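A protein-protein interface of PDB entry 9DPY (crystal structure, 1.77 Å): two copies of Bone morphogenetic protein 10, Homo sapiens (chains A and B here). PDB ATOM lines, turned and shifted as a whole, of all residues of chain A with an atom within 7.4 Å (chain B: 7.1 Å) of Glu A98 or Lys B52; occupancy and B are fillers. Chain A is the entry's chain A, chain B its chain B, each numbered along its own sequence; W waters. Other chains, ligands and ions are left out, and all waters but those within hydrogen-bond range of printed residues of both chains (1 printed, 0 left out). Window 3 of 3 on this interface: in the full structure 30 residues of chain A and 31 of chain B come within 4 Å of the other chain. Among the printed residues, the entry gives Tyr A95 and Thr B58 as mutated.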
ATOM      1  N   TRP A  21     -15.539  25.673 -12.859  1.00  0.00           N
ATOM      2  CA  TRP A  21     -15.396  25.802 -14.300  1.00  0.00           C
ATOM      3  C   TRP A  21     -15.476  27.244 -14.776  1.00  0.00           C
ATOM      4  O   TRP A  21     -15.251  27.492 -15.968  1.00  0.00           O
ATOM      5  CB  TRP A  21     -16.443  24.964 -15.032  1.00  0.00           C
ATOM      6  CG  TRP A  21     -16.050  23.520 -15.051  1.00  0.00           C
ATOM      7  CD1 TRP A  21     -15.109  22.917 -14.256  1.00  0.00           C
ATOM      8  CD2 TRP A  21     -16.562  22.500 -15.908  1.00  0.00           C
ATOM      9  NE1 TRP A  21     -15.000  21.591 -14.578  1.00  0.00           N
ATOM     10  CE2 TRP A  21     -15.890  21.302 -15.579  1.00  0.00           C
ATOM     11  CE3 TRP A  21     -17.524  22.476 -16.922  1.00  0.00           C
ATOM     12  CZ2 TRP A  21     -16.152  20.098 -16.225  1.00  0.00           C
ATOM     13  CZ3 TRP A  21     -17.778  21.274 -17.570  1.00  0.00           C
ATOM     14  CH2 TRP A  21     -17.092  20.105 -17.219  1.00  0.00           C
ATOM     15  N   TRP A  24     -12.549  28.633 -16.998  1.00  0.00           N
ATOM     16  CA  TRP A  24     -12.416  28.590 -18.443  1.00  0.00           C
ATOM     17  C   TRP A  24     -13.709  28.836 -19.198  1.00  0.00           C
ATOM     18  O   TRP A  24     -13.646  29.137 -20.395  1.00  0.00           O
ATOM     19  CB  TRP A  24     -11.817  27.244 -18.900  1.00  0.00           C
ATOM     20  CG  TRP A  24     -12.673  26.043 -18.571  1.00  0.00           C
ATOM     21  CD1 TRP A  24     -12.801  25.440 -17.348  1.00  0.00           C
ATOM     22  CD2 TRP A  24     -13.496  25.298 -19.475  1.00  0.00           C
ATOM     23  NE1 TRP A  24     -13.657  24.373 -17.444  1.00  0.00           N
ATOM     24  CE2 TRP A  24     -14.101  24.266 -18.733  1.00  0.00           C
ATOM     25  CE3 TRP A  24     -13.786  25.404 -20.838  1.00  0.00           C
ATOM     26  CZ2 TRP A  24     -14.976  23.350 -19.310  1.00  0.00           C
ATOM     27  CZ3 TRP A  24     -14.653  24.496 -21.406  1.00  0.00           C
ATOM     28  CH2 TRP A  24     -15.238  23.480 -20.640  1.00  0.00           C
ATOM     29  N   TYR A  31     -26.425  26.823 -16.184  1.00  0.00           N
ATOM     30  CA  TYR A  31     -27.445  26.350 -17.109  1.00  0.00           C
ATOM     31  C   TYR A  31     -28.295  25.290 -16.414  1.00  0.00           C
ATOM     32  O   TYR A  31     -27.937  24.778 -15.349  1.00  0.00           O
ATOM     33  CB  TYR A  31     -26.828  25.796 -18.399  1.00  0.00           C
ATOM     34  CG  TYR A  31     -26.182  24.422 -18.256  1.00  0.00           C
ATOM     35  CD1 TYR A  31     -24.992  24.256 -17.557  1.00  0.00           C
ATOM     36  CD2 TYR A  31     -26.764  23.299 -18.829  1.00  0.00           C
ATOM     37  CE1 TYR A  31     -24.401  23.000 -17.434  1.00  0.00           C
ATOM     38  CE2 TYR A  31     -26.179  22.061 -18.732  1.00  0.00           C
ATOM     39  CZ  TYR A  31     -25.004  21.904 -18.037  1.00  0.00           C
ATOM     40  OH  TYR A  31     -24.436  20.643 -17.921  1.00  0.00           O
ATOM     41  N   LEU A  78     -29.050  13.363 -24.476  1.00  0.00           N
ATOM     42  CA  LEU A  78     -28.421  14.577 -23.970  1.00  0.00           C
ATOM     43  C   LEU A  78     -28.478  15.650 -25.053  1.00  0.00           C
ATOM     44  O   LEU A  78     -28.424  15.344 -26.247  1.00  0.00           O
ATOM     45  CB  LEU A  78     -26.977  14.309 -23.572  1.00  0.00           C
ATOM     46  CG  LEU A  78     -26.794  13.379 -22.374  1.00  0.00           C
ATOM     47  CD1 LEU A  78     -25.339  12.999 -22.246  1.00  0.00           C
ATOM     48  CD2 LEU A  78     -27.264  14.080 -21.112  1.00  0.00           C
ATOM     49  N   GLU A  79     -28.606  16.909 -24.629  1.00  0.00           N
ATOM     50  CA  GLU A  79     -28.705  18.029 -25.555  1.00  0.00           C
ATOM     51  C   GLU A  79     -27.510  18.962 -25.399  1.00  0.00           C
ATOM     52  O   GLU A  79     -26.953  19.078 -24.303  1.00  0.00           O
ATOM     53  CB  GLU A  79     -29.978  18.852 -25.318  1.00  0.00           C
ATOM     54  CG  GLU A  79     -31.268  18.045 -25.377  1.00  0.00           C
ATOM     55  CD  GLU A  79     -31.580  17.504 -26.761  1.00  0.00           C
ATOM     56  OE1 GLU A  79     -30.906  17.894 -27.737  1.00  0.00           O
ATOM     57  OE2 GLU A  79     -32.513  16.681 -26.873  1.00  0.00           O
ATOM     58  N   PRO A  80     -27.127  19.680 -26.453  1.00  0.00           N
ATOM     59  CA  PRO A  80     -26.045  20.661 -26.321  1.00  0.00           C
ATOM     60  C   PRO A  80     -26.522  21.975 -25.716  1.00  0.00           C
ATOM     61  O   PRO A  80     -27.717  22.261 -25.640  1.00  0.00           O
ATOM     62  CB  PRO A  80     -25.584  20.865 -27.770  1.00  0.00           C
ATOM     63  CG  PRO A  80     -26.829  20.640 -28.574  1.00  0.00           C
ATOM     64  CD  PRO A  80     -27.608  19.572 -27.847  1.00  0.00           C
ATOM     65  N   ILE A  81     -25.549  22.778 -25.273  1.00  0.00           N
ATOM     66  CA  ILE A  81     -25.759  24.200 -25.011  1.00  0.00           C
ATOM     67  C   ILE A  81     -24.682  24.990 -25.751  1.00  0.00           C
ATOM     68  O   ILE A  81     -23.658  24.445 -26.169  1.00  0.00           O
ATOM     69  CB  ILE A  81     -25.726  24.552 -23.501  1.00  0.00           C
ATOM     70  CG1 ILE A  81     -24.310  24.368 -22.937  1.00  0.00           C
ATOM     71  CG2 ILE A  81     -26.738  23.718 -22.721  1.00  0.00           C
ATOM     72  CD1 ILE A  81     -24.134  24.908 -21.519  1.00  0.00           C
ATOM     73  N   LYS A  94     -18.747  28.147 -29.228  1.00  0.00           N
ATOM     74  CA  LYS A  94     -19.283  26.884 -29.724  1.00  0.00           C
ATOM     75  C   LYS A  94     -20.787  26.888 -29.497  1.00  0.00           C
ATOM     76  O   LYS A  94     -21.244  26.840 -28.346  1.00  0.00           O
ATOM     77  CB  LYS A  94     -18.628  25.690 -29.037  1.00  0.00           C
ATOM     78  CG  LYS A  94     -19.042  24.358 -29.663  1.00  0.00           C
ATOM     79  CD  LYS A  94     -17.947  23.317 -29.505  1.00  0.00           C
ATOM     80  CE  LYS A  94     -18.322  22.024 -30.212  1.00  0.00           C
ATOM     81  NZ  LYS A  94     -18.658  22.251 -31.646  1.00  0.00           N
ATOM     82  N   TYR A  95     -21.551  26.918 -30.594  1.00  0.00           N
ATOM     83  CA  TYR A  95     -23.004  27.001 -30.497  1.00  0.00           C
ATOM     84  C   TYR A  95     -23.618  25.732 -29.930  1.00  0.00           C
ATOM     85  O   TYR A  95     -24.648  25.803 -29.256  1.00  0.00           O
ATOM     86  CB  TYR A  95     -23.636  27.273 -31.864  1.00  0.00           C
ATOM     87  CG  TYR A  95     -23.482  28.702 -32.328  1.00  0.00           C
ATOM     88  CD1 TYR A  95     -23.483  29.757 -31.419  1.00  0.00           C
ATOM     89  CD2 TYR A  95     -23.352  29.005 -33.691  1.00  0.00           C
ATOM     90  CE1 TYR A  95     -23.331  31.099 -31.866  1.00  0.00           C
ATOM     91  CE2 TYR A  95     -23.215  30.326 -34.141  1.00  0.00           C
ATOM     92  CZ  TYR A  95     -23.214  31.359 -33.227  1.00  0.00           C
ATOM     93  OH  TYR A  95     -23.077  32.671 -33.693  1.00  0.00           O
ATOM     94  N   LYS A  96     -23.044  24.564 -30.222  1.00  0.00           N
ATOM     95  CA  LYS A  96     -23.569  23.304 -29.683  1.00  0.00           C
ATOM     96  C   LYS A  96     -22.440  22.471 -29.073  1.00  0.00           C
ATOM     97  O   LYS A  96     -21.845  21.607 -29.723  1.00  0.00           O
ATOM     98  CB  LYS A  96     -24.354  22.515 -30.751  1.00  0.00           C
ATOM     99  CG  LYS A  96     -23.704  22.385 -32.114  1.00  0.00           C
ATOM    100  CD  LYS A  96     -24.560  21.544 -33.048  1.00  0.00           C
ATOM    101  CE  LYS A  96     -25.970  22.104 -33.157  1.00  0.00           C
ATOM    102  NZ  LYS A  96     -26.844  21.250 -34.010  1.00  0.00           N
ATOM    103  N   TYR A  97     -22.168  22.734 -27.799  1.00  0.00           N
ATOM    104  CA  TYR A  97     -21.256  21.939 -26.986  1.00  0.00           C
ATOM    105  C   TYR A  97     -22.052  20.732 -26.484  1.00  0.00           C
ATOM    106  O   TYR A  97     -22.935  20.875 -25.635  1.00  0.00           O
ATOM    107  CB  TYR A  97     -20.718  22.816 -25.857  1.00  0.00           C
ATOM    108  CG  TYR A  97     -19.510  22.289 -25.096  1.00  0.00           C
ATOM    109  CD1 TYR A  97     -18.237  22.275 -25.664  1.00  0.00           C
ATOM    110  CD2 TYR A  97     -19.646  21.841 -23.790  1.00  0.00           C
ATOM    111  CE1 TYR A  97     -17.144  21.811 -24.957  1.00  0.00           C
ATOM    112  CE2 TYR A  97     -18.556  21.380 -23.076  1.00  0.00           C
ATOM    113  CZ  TYR A  97     -17.310  21.365 -23.663  1.00  0.00           C
ATOM    114  OH  TYR A  97     -16.225  20.903 -22.954  1.00  0.00           O
ATOM    115  N   GLU A  98     -21.768  19.551 -27.029  1.00  0.00           N
ATOM    116  CA  GLU A  98     -22.674  18.413 -26.898  1.00  0.00           C
ATOM    117  C   GLU A  98     -22.626  17.769 -25.511  1.00  0.00           C
ATOM    118  O   GLU A  98     -21.649  17.875 -24.765  1.00  0.00           O
ATOM    119  CB  GLU A  98     -22.340  17.340 -27.940  1.00  0.00           C
ATOM    120  CG  GLU A  98     -22.447  17.844 -29.402  1.00  0.00           C
ATOM    121  CD  GLU A  98     -23.879  17.923 -29.903  1.00  0.00           C
ATOM    122  OE1 GLU A  98     -24.791  17.396 -29.209  1.00  0.00           O
ATOM    123  OE2 GLU A  98     -24.101  18.501 -30.987  1.00  0.00           O
ATOM    124  N   GLY A  99     -23.707  17.062 -25.186  1.00  0.00           N
ATOM    125  CA  GLY A  99     -23.709  16.186 -24.033  1.00  0.00           C
ATOM    126  C   GLY A  99     -24.030  16.825 -22.704  1.00  0.00           C
ATOM    127  O   GLY A  99     -23.732  16.225 -21.666  1.00  0.00           O
ATOM    128  N   MET A 100     -24.693  17.982 -22.687  1.00  0.00           N
ATOM    129  CA  MET A 100     -24.711  18.793 -21.474  1.00  0.00           C
ATOM    130  C   MET A 100     -26.006  18.735 -20.673  1.00  0.00           C
ATOM    131  O   MET A 100     -25.955  18.796 -19.439  1.00  0.00           O
ATOM    132  CB  MET A 100     -24.419  20.257 -21.819  1.00  0.00           C
ATOM    133  CG  MET A 100     -23.005  20.472 -22.378  1.00  0.00           C
ATOM    134  SD  MET A 100     -21.756  20.362 -21.088  1.00  0.00           S
ATOM    135  CE  MET A 100     -22.062  21.879 -20.174  1.00  0.00           C
ATOM    136  N   ALA A 101     -27.161  18.661 -21.327  1.00  0.00           N
ATOM    137  CA  ALA A 101     -28.448  18.783 -20.653  1.00  0.00           C
ATOM    138  C   ALA A 101     -29.265  17.535 -20.933  1.00  0.00           C
ATOM    139  O   ALA A 101     -29.332  17.091 -22.082  1.00  0.00           O
ATOM    140  CB  ALA A 101     -29.236  20.008 -21.127  1.00  0.00           C
ATOM    141  N   THR B  49     -15.887   6.079 -20.610  1.00  0.00           N
ATOM    142  CA  THR B  49     -16.486   6.973 -21.601  1.00  0.00           C
ATOM    143  C   THR B  49     -17.525   7.918 -21.011  1.00  0.00           C
ATOM    144  O   THR B  49     -18.626   8.052 -21.559  1.00  0.00           O
ATOM    145  CB  THR B  49     -17.125   6.176 -22.751  1.00  0.00           C
ATOM    146  OG1 THR B  49     -18.172   5.317 -22.270  1.00  0.00           O
ATOM    147  CG2 THR B  49     -16.081   5.322 -23.451  1.00  0.00           C
ATOM    148  N   PRO B  50     -17.204   8.636 -19.943  1.00  0.00           N
ATOM    149  CA  PRO B  50     -18.207   9.521 -19.343  1.00  0.00           C
ATOM    150  C   PRO B  50     -18.650  10.618 -20.305  1.00  0.00           C
ATOM    151  O   PRO B  50     -17.849  11.197 -21.050  1.00  0.00           O
ATOM    152  CB  PRO B  50     -17.486  10.093 -18.114  1.00  0.00           C
ATOM    153  CG  PRO B  50     -16.032  10.051 -18.499  1.00  0.00           C
ATOM    154  CD  PRO B  50     -15.889   8.764 -19.287  1.00  0.00           C
ATOM    155  N   THR B  51     -19.952  10.875 -20.299  1.00  0.00           N
ATOM    156  CA  THR B  51     -20.500  12.046 -20.956  1.00  0.00           C
ATOM    157  C   THR B  51     -20.081  13.313 -20.204  1.00  0.00           C
ATOM    158  O   THR B  51     -19.646  13.276 -19.046  1.00  0.00           O
ATOM    159  CB  THR B  51     -22.024  11.966 -21.000  1.00  0.00           C
ATOM    160  OG1 THR B  51     -22.518  11.859 -19.652  1.00  0.00           O
ATOM    161  CG2 THR B  51     -22.505  10.761 -21.840  1.00  0.00           C
ATOM    162  N   LYS B  52     -20.267  14.461 -20.862  1.00  0.00           N
ATOM    163  CA  LYS B  52     -20.008  15.720 -20.176  1.00  0.00           C
ATOM    164  C   LYS B  52     -20.987  15.901 -19.022  1.00  0.00           C
ATOM    165  O   LYS B  52     -20.611  16.368 -17.945  1.00  0.00           O
ATOM    166  CB  LYS B  52     -20.072  16.877 -21.176  1.00  0.00           C
ATOM    167  CG  LYS B  52     -19.095  16.681 -22.363  1.00  0.00           C
ATOM    168  CD  LYS B  52     -18.784  17.967 -23.085  1.00  0.00           C
ATOM    169  CE  LYS B  52     -18.151  17.750 -24.443  1.00  0.00           C
ATOM    170  NZ  LYS B  52     -19.064  18.128 -25.546  1.00  0.00           N
ATOM    171  N   HIS B  53     -22.236  15.472 -19.207  1.00  0.00           N
ATOM    172  CA  HIS B  53     -23.211  15.600 -18.131  1.00  0.00           C
ATOM    173  C   HIS B  53     -22.803  14.764 -16.923  1.00  0.00           C
ATOM    174  O   HIS B  53     -22.901  15.218 -15.776  1.00  0.00           O
ATOM    175  CB  HIS B  53     -24.599  15.197 -18.628  1.00  0.00           C
ATOM    176  CG  HIS B  53     -25.674  15.437 -17.616  1.00  0.00           C
ATOM    177  ND1 HIS B  53     -25.953  14.542 -16.604  1.00  0.00           N
ATOM    178  CD2 HIS B  53     -26.512  16.484 -17.434  1.00  0.00           C
ATOM    179  CE1 HIS B  53     -26.933  15.017 -15.854  1.00  0.00           C
ATOM    180  NE2 HIS B  53     -27.292  16.195 -16.340  1.00  0.00           N
ATOM    181  N   ALA B  54     -22.299  13.555 -17.161  1.00  0.00           N
ATOM    182  CA  ALA B  54     -21.871  12.715 -16.048  1.00  0.00           C
ATOM    183  C   ALA B  54     -20.681  13.327 -15.322  1.00  0.00           C
ATOM    184  O   ALA B  54     -20.569  13.217 -14.093  1.00  0.00           O
ATOM    185  CB  ALA B  54     -21.533  11.309 -16.545  1.00  0.00           C
ATOM    186  N   ILE B  55     -19.773  13.956 -16.062  1.00  0.00           N
ATOM    187  CA  ILE B  55     -18.637  14.624 -15.430  1.00  0.00           C
ATOM    188  C   ILE B  55     -19.124  15.778 -14.563  1.00  0.00           C
ATOM    189  O   ILE B  55     -18.707  15.929 -13.411  1.00  0.00           O
ATOM    190  CB  ILE B  55     -17.634  15.102 -16.495  1.00  0.00           C
ATOM    191  CG1 ILE B  55     -16.916  13.905 -17.126  1.00  0.00           C
ATOM    192  CG2 ILE B  55     -16.621  16.068 -15.877  1.00  0.00           C
ATOM    193  CD1 ILE B  55     -16.351  14.175 -18.527  1.00  0.00           C
ATOM    194  N   ILE B  56     -20.011  16.614 -15.102  1.00  0.00           N
ATOM    195  CA  ILE B  56     -20.451  17.792 -14.357  1.00  0.00           C
ATOM    196  C   ILE B  56     -21.323  17.392 -13.176  1.00  0.00           C
ATOM    197  O   ILE B  56     -21.249  17.992 -12.100  1.00  0.00           O
ATOM    198  CB  ILE B  56     -21.188  18.766 -15.289  1.00  0.00           C
ATOM    199  CG1 ILE B  56     -20.307  19.110 -16.494  1.00  0.00           C
ATOM    200  CG2 ILE B  56     -21.516  20.050 -14.558  1.00  0.00           C
ATOM    201  CD1 ILE B  56     -21.020  19.897 -17.540  1.00  0.00           C
ATOM    202  N   GLN B  57     -22.188  16.400 -13.361  1.00  0.00           N
ATOM    203  CA  GLN B  57     -22.982  15.915 -12.234  1.00  0.00           C
ATOM    204  C   GLN B  57     -22.087  15.370 -11.129  1.00  0.00           C
ATOM    205  O   GLN B  57     -22.315  15.630  -9.938  1.00  0.00           O
ATOM    206  CB  GLN B  57     -23.954  14.844 -12.731  1.00  0.00           C
ATOM    207  CG  GLN B  57     -24.920  14.354 -11.680  1.00  0.00           C
ATOM    208  CD  GLN B  57     -25.813  13.265 -12.209  1.00  0.00           C
ATOM    209  OE1 GLN B  57     -26.473  13.423 -13.252  1.00  0.00           O
ATOM    210  NE2 GLN B  57     -25.853  12.142 -11.502  1.00  0.00           N
ATOM    211  N   THR B  58     -21.055  14.621 -11.503  1.00  0.00           N
ATOM    212  CA  THR B  58     -20.153  14.077 -10.501  1.00  0.00           C
ATOM    213  C   THR B  58     -19.461  15.191  -9.731  1.00  0.00           C
ATOM    214  O   THR B  58     -19.289  15.096  -8.511  1.00  0.00           O
ATOM    215  CB  THR B  58     -19.124  13.161 -11.165  1.00  0.00           C
ATOM    216  OG1 THR B  58     -19.789  12.028 -11.741  1.00  0.00           O
ATOM    217  CG2 THR B  58     -18.095  12.659 -10.156  1.00  0.00           C
HETATM  218  O   HOH W   1     -18.910  19.020 -28.315  1.00  0.00           O
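Of the printed residues of chain B, Trp A21 touches Ile B56. Of the printed residues of chain B, Leu A78 touches Thr B51 and His B53. Printed residues of chain B within 4 Å of Tyr A97: Lys B52. Of the printed residues of chain B, Glu A98 touches Lys B52 (2.7 Å). Pro B50 touches none of the printed residues of chain A. Printed residues of chain A within 4 Å of Thr B51: Leu A78. Of chain A, only Tyr A97, Glu A98, Gly A99 and Met A100 come within 4 Å of Lys B52. Printed residues of chain A within 4 Å of Ile B56: Trp A21, Tyr A31 and Met A100. The nearest residue of chain B that does not touch Glu A98 is His B53 (6.1 Å). The nearest residue of chain A that does not touch Lys B52 is Trp A21 (5.2 Å).
Of the 10 printed residues of chain B, 4 touch a printed residue of chain A. Hydrophobic or aromatic side chains of chain A within 4 Å of the printed part of chain B: Trp A21, Tyr A31, Leu A78, Tyr A97 and Met A100. Among the printed residues, no Asp or Glu carboxylate lies within 4 Å of a Lys or Arg side-chain nitrogen of the other chain.
Water W1 bridges the side-chain amino group of Lys B52 and the backbone NH of Glu A98.
No position is printed for both chains.
O of Glu A79 is in hydrogen-bond range of N of Met A100, 3.0 Å away. The side-chain hydroxyl (OH) of Tyr A31 sits at hydrogen-bond distance from the backbone carbonyl oxygen (O) of Met A100, 2.8 Å away. The backbone NH (N) of Ala B54 sits at hydrogen-bond distance from the side-chain hydroxyl (OG1) of Thr B51. The backbone carbonyl oxygen of Ile A81 lies within hydrogen-bond range of the backbone NH of Tyr A97 (2.8 Å).
CH2 of Trp A21 touches CG1 of Ile B56, 3.4 Å away. Ile B56 touches Tyr A31 (CD1 to OH, 3.5 Å). Leu A78 touches Thr B51 (CD1 to CG2, 3.6 Å). CD2 of Leu A78 touches CB of His B53, 3.8 Å away. Tyr A97 touches Lys B52 (CE2 to CD, 3.4 Å). Lys B52 touches Gly A99. Met A100 touches Lys B52 (SD to CB, 3.9 Å). Met A100 touches His B53. CE of Met A100 touches CD1 of Ile B56, at 3.5 Å.
The backbone carbonyl oxygen (O) of Gly A99 sits at hydrogen-bond distance from the backbone NH (N) of His B53, at 3.0 Å. NZ of Lys B52 sits at hydrogen-bond distance from O of Glu A98, at 2.7 Å.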
